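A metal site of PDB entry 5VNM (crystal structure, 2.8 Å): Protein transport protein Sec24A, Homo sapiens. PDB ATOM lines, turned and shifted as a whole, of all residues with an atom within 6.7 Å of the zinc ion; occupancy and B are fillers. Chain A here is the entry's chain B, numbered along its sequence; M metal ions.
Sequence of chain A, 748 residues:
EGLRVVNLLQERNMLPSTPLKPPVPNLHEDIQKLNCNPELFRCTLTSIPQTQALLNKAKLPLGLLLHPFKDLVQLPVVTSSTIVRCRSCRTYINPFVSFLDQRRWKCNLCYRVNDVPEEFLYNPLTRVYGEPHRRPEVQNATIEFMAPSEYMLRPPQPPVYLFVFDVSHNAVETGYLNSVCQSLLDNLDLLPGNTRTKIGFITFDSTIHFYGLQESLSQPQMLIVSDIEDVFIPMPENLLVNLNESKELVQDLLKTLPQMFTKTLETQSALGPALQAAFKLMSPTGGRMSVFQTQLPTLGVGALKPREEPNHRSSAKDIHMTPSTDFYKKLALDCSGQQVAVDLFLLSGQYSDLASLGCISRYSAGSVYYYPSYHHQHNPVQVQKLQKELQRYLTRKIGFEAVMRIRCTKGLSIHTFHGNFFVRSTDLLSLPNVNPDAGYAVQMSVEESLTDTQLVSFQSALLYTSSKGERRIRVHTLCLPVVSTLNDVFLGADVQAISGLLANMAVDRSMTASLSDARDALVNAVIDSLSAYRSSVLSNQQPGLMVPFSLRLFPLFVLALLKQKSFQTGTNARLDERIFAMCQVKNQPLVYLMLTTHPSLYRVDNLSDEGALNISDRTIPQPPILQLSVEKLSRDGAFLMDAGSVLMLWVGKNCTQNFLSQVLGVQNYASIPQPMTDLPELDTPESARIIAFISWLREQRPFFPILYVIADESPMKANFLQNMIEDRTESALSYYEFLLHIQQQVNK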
ATOM      1  N   CYS A  86     -21.745 -22.082   0.413  1.00  0.00           N
ATOM      2  CA  CYS A  86     -22.988 -21.832  -0.306  1.00  0.00           C
ATOM      3  C   CYS A  86     -23.550 -23.131  -0.867  1.00  0.00           C
ATOM      4  O   CYS A  86     -22.824 -23.914  -1.478  1.00  0.00           O
ATOM      5  CB  CYS A  86     -22.756 -20.822  -1.427  1.00  0.00           C
ATOM      6  SG  CYS A  86     -24.099 -20.736  -2.636  1.00  0.00           S
ATOM      7  N   ARG A  87     -24.848 -23.343  -0.674  1.00  0.00           N
ATOM      8  CA  ARG A  87     -25.480 -24.598  -1.070  1.00  0.00           C
ATOM      9  C   ARG A  87     -25.510 -24.806  -2.575  1.00  0.00           C
ATOM     10  O   ARG A  87     -25.825 -25.912  -3.029  1.00  0.00           O
ATOM     11  CB  ARG A  87     -26.907 -24.663  -0.526  1.00  0.00           C
ATOM     12  CG  ARG A  87     -27.000 -24.792   0.995  1.00  0.00           C
ATOM     13  CD  ARG A  87     -28.443 -24.914   1.447  1.00  0.00           C
ATOM     14  NE  ARG A  87     -28.573 -24.994   2.895  1.00  0.00           N
ATOM     15  CZ  ARG A  87     -29.724 -25.162   3.538  1.00  0.00           C
ATOM     16  NH1 ARG A  87     -30.856 -25.245   2.858  1.00  0.00           N
ATOM     17  NH2 ARG A  87     -29.752 -25.231   4.863  1.00  0.00           N
ATOM     18  N   SER A  88     -25.192 -23.776  -3.372  1.00  0.00           N
ATOM     19  CA  SER A  88     -25.233 -23.920  -4.828  1.00  0.00           C
ATOM     20  C   SER A  88     -23.841 -24.142  -5.410  1.00  0.00           C
ATOM     21  O   SER A  88     -23.510 -25.260  -5.831  1.00  0.00           O
ATOM     22  CB  SER A  88     -25.873 -22.690  -5.469  1.00  0.00           C
ATOM     23  OG  SER A  88     -27.276 -22.692  -5.276  1.00  0.00           O
ATOM     24  N   CYS A  89     -23.018 -23.100  -5.434  1.00  0.00           N
ATOM     25  CA  CYS A  89     -21.694 -23.152  -6.056  1.00  0.00           C
ATOM     26  C   CYS A  89     -20.593 -23.538  -5.085  1.00  0.00           C
ATOM     27  O   CYS A  89     -19.413 -23.514  -5.464  1.00  0.00           O
ATOM     28  CB  CYS A  89     -21.369 -21.803  -6.714  1.00  0.00           C
ATOM     29  SG  CYS A  89     -21.345 -20.405  -5.564  1.00  0.00           S
ATOM     30  N   ARG A  90     -20.945 -23.883  -3.841  1.00  0.00           N
ATOM     31  CA  ARG A  90     -19.976 -24.340  -2.831  1.00  0.00           C
ATOM     32  C   ARG A  90     -18.922 -23.286  -2.514  1.00  0.00           C
ATOM     33  O   ARG A  90     -17.786 -23.621  -2.175  1.00  0.00           O
ATOM     34  CB  ARG A  90     -19.306 -25.658  -3.253  1.00  0.00           C
ATOM     35  CG  ARG A  90     -20.275 -26.787  -3.562  1.00  0.00           C
ATOM     36  CD  ARG A  90     -21.349 -26.943  -2.485  1.00  0.00           C
ATOM     37  NE  ARG A  90     -20.796 -27.001  -1.141  1.00  0.00           N
ATOM     38  CZ  ARG A  90     -20.383 -28.110  -0.539  1.00  0.00           C
ATOM     39  NH1 ARG A  90     -20.477 -29.278  -1.167  1.00  0.00           N
ATOM     40  NH2 ARG A  90     -19.904 -28.059   0.698  1.00  0.00           N
ATOM     41  N   THR A  91     -19.277 -22.008  -2.628  1.00  0.00           N
ATOM     42  CA  THR A  91     -18.353 -20.933  -2.297  1.00  0.00           C
ATOM     43  C   THR A  91     -18.280 -20.763  -0.788  1.00  0.00           C
ATOM     44  O   THR A  91     -19.303 -20.701  -0.106  1.00  0.00           O
ATOM     45  CB  THR A  91     -18.798 -19.630  -2.963  1.00  0.00           C
ATOM     46  OG1 THR A  91     -18.774 -19.780  -4.389  1.00  0.00           O
ATOM     47  CG2 THR A  91     -17.871 -18.489  -2.558  1.00  0.00           C
ATOM     48  N   TRP A 105     -27.513 -15.133   4.365  1.00  0.00           N
ATOM     49  CA  TRP A 105     -26.481 -14.392   3.651  1.00  0.00           C
ATOM     50  C   TRP A 105     -26.580 -14.671   2.157  1.00  0.00           C
ATOM     51  O   TRP A 105     -26.841 -15.810   1.741  1.00  0.00           O
ATOM     52  CB  TRP A 105     -25.073 -14.747   4.166  1.00  0.00           C
ATOM     53  CG  TRP A 105     -24.699 -16.197   4.032  1.00  0.00           C
ATOM     54  CD1 TRP A 105     -25.052 -17.208   4.880  1.00  0.00           C
ATOM     55  CD2 TRP A 105     -23.872 -16.782   3.024  1.00  0.00           C
ATOM     56  NE1 TRP A 105     -24.513 -18.392   4.437  1.00  0.00           N
ATOM     57  CE2 TRP A 105     -23.784 -18.160   3.310  1.00  0.00           C
ATOM     58  CE3 TRP A 105     -23.203 -16.291   1.900  1.00  0.00           C
ATOM     59  CZ2 TRP A 105     -23.055 -19.043   2.519  1.00  0.00           C
ATOM     60  CZ3 TRP A 105     -22.482 -17.160   1.112  1.00  0.00           C
ATOM     61  CH2 TRP A 105     -22.409 -18.524   1.421  1.00  0.00           C
ATOM     62  N   CYS A 107     -24.926 -15.165  -1.390  1.00  0.00           N
ATOM     63  CA  CYS A 107     -23.662 -15.555  -1.991  1.00  0.00           C
ATOM     64  C   CYS A 107     -23.190 -14.499  -2.982  1.00  0.00           C
ATOM     65  O   CYS A 107     -23.952 -14.071  -3.852  1.00  0.00           O
ATOM     66  CB  CYS A 107     -23.816 -16.912  -2.692  1.00  0.00           C
ATOM     67  SG  CYS A 107     -22.318 -17.577  -3.457  1.00  0.00           S
ATOM     68  N   ASN A 108     -21.942 -14.065  -2.833  1.00  0.00           N
ATOM     69  CA  ASN A 108     -21.405 -13.036  -3.719  1.00  0.00           C
ATOM     70  C   ASN A 108     -20.887 -13.594  -5.036  1.00  0.00           C
ATOM     71  O   ASN A 108     -20.334 -12.825  -5.836  1.00  0.00           O
ATOM     72  CB  ASN A 108     -20.287 -12.255  -3.001  1.00  0.00           C
ATOM     73  CG  ASN A 108     -19.196 -13.160  -2.467  1.00  0.00           C
ATOM     74  OD1 ASN A 108     -19.461 -14.291  -2.047  1.00  0.00           O
ATOM     75  ND2 ASN A 108     -17.962 -12.668  -2.478  1.00  0.00           N
ATOM     76  N   LEU A 109     -21.053 -14.888  -5.289  1.00  0.00           N
ATOM     77  CA  LEU A 109     -20.599 -15.499  -6.535  1.00  0.00           C
ATOM     78  C   LEU A 109     -21.723 -16.118  -7.352  1.00  0.00           C
ATOM     79  O   LEU A 109     -21.610 -16.164  -8.577  1.00  0.00           O
ATOM     80  CB  LEU A 109     -19.532 -16.571  -6.249  1.00  0.00           C
ATOM     81  CG  LEU A 109     -18.065 -16.128  -6.271  1.00  0.00           C
ATOM     82  CD1 LEU A 109     -17.804 -15.064  -5.217  1.00  0.00           C
ATOM     83  CD2 LEU A 109     -17.159 -17.314  -6.057  1.00  0.00           C
ATOM     84  N   CYS A 110     -22.794 -16.599  -6.719  1.00  0.00           N
ATOM     85  CA  CYS A 110     -23.932 -17.151  -7.445  1.00  0.00           C
ATOM     86  C   CYS A 110     -25.267 -16.561  -6.975  1.00  0.00           C
ATOM     87  O   CYS A 110     -26.323 -17.019  -7.430  1.00  0.00           O
ATOM     88  CB  CYS A 110     -23.974 -18.678  -7.342  1.00  0.00           C
ATOM     89  SG  CYS A 110     -24.772 -19.309  -5.851  1.00  0.00           S
ATOM     90  N   TYR A 111     -25.239 -15.586  -6.075  1.00  0.00           N
ATOM     91  CA  TYR A 111     -26.366 -14.759  -5.659  1.00  0.00           C
ATOM     92  C   TYR A 111     -27.438 -15.520  -4.881  1.00  0.00           C
ATOM     93  O   TYR A 111     -28.437 -14.915  -4.476  1.00  0.00           O
ATOM     94  CB  TYR A 111     -27.035 -14.048  -6.840  1.00  0.00           C
ATOM     95  CG  TYR A 111     -26.052 -13.277  -7.699  1.00  0.00           C
ATOM     96  CD1 TYR A 111     -24.994 -12.584  -7.127  1.00  0.00           C
ATOM     97  CD2 TYR A 111     -26.175 -13.267  -9.083  1.00  0.00           C
ATOM     98  CE1 TYR A 111     -24.091 -11.882  -7.913  1.00  0.00           C
ATOM     99  CE2 TYR A 111     -25.273 -12.578  -9.875  1.00  0.00           C
ATOM    100  CZ  TYR A 111     -24.241 -11.881  -9.288  1.00  0.00           C
ATOM    101  OH  TYR A 111     -23.354 -11.194 -10.072  1.00  0.00           O
ATOM    102  N   ARG A 112     -27.266 -16.824  -4.648  1.00  0.00           N
ATOM    103  CA  ARG A 112     -28.238 -17.563  -3.854  1.00  0.00           C
ATOM    104  C   ARG A 112     -28.136 -17.180  -2.378  1.00  0.00           C
ATOM    105  O   ARG A 112     -27.035 -16.975  -1.854  1.00  0.00           O
ATOM    106  CB  ARG A 112     -28.042 -19.064  -4.022  1.00  0.00           C
ATOM    107  CG  ARG A 112     -28.426 -19.879  -2.786  1.00  0.00           C
ATOM    108  CD  ARG A 112     -29.019 -21.232  -3.122  1.00  0.00           C
ATOM    109  NE  ARG A 112     -29.586 -21.867  -1.936  1.00  0.00           N
ATOM    110  CZ  ARG A 112     -30.050 -23.103  -1.900  1.00  0.00           C
ATOM    111  NH1 ARG A 112     -30.003 -23.863  -2.988  1.00  0.00           N
ATOM    112  NH2 ARG A 112     -30.552 -23.593  -0.779  1.00  0.00           N
ATOM    113  N   ASN A 114     -28.336 -18.132   1.491  1.00  0.00           N
ATOM    114  CA  ASN A 114     -28.084 -19.318   2.293  1.00  0.00           C
ATOM    115  C   ASN A 114     -28.439 -19.049   3.755  1.00  0.00           C
ATOM    116  O   ASN A 114     -28.444 -17.904   4.213  1.00  0.00           O
ATOM    117  CB  ASN A 114     -26.619 -19.758   2.193  1.00  0.00           C
ATOM    118  CG  ASN A 114     -26.317 -20.453   0.877  1.00  0.00           C
ATOM    119  OD1 ASN A 114     -26.522 -21.652   0.742  1.00  0.00           O
ATOM    120  ND2 ASN A 114     -25.826 -19.689  -0.091  1.00  0.00           N
HETATM  121 ZN    ZN M   1     -23.105 -19.578  -4.344  1.00  0.00          ZN
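The zinc ion is bound by the side-chain sulfur of Cys 110 (2.3 Å), the side-chain sulfur of Cys 86 (2.3 Å), the side-chain sulfur of Cys 89 (2.3 Å) and the side-chain sulfur of Cys 107 (2.3 Å).
Four residues have an atom within 4 Å of the zinc ion: Cys 86, Cys 89, Cys 107 and Cys 110.
The nearest printed residue that does not touch the zinc ion is Ser 88 (4.3 Å).
The side-chain amide nitrogen (ND2) of Asn 114 sits close to the side-chain sulfur (SG) of Cys 86, at 3.2 Å.
The backbone NH (N) of Cys 86 lies within hydrogen-bond range of the backbone carbonyl oxygen (O) of Thr 91 (2.9 Å).
The backbone NH (N) of Cys 107 is in hydrogen-bond range of the backbone carbonyl oxygen (O) of Arg 112 (2.8 Å).
The backbone NH (N) of Leu 109 sits close to the side-chain sulfur (SG) of Cys 107.
The side-chain hydroxyl (OG1) of Thr 91 lies close to the side-chain sulfur (SG) of Cys 89 (2.9 Å).
The backbone NH (N) of Arg 112 sits close to the side-chain sulfur (SG) of Cys 110 (3.7 Å).
The side-chain sulfur (SG) of Cys 86 lies close to the backbone NH (N) of Ser 88 (3.3 Å).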
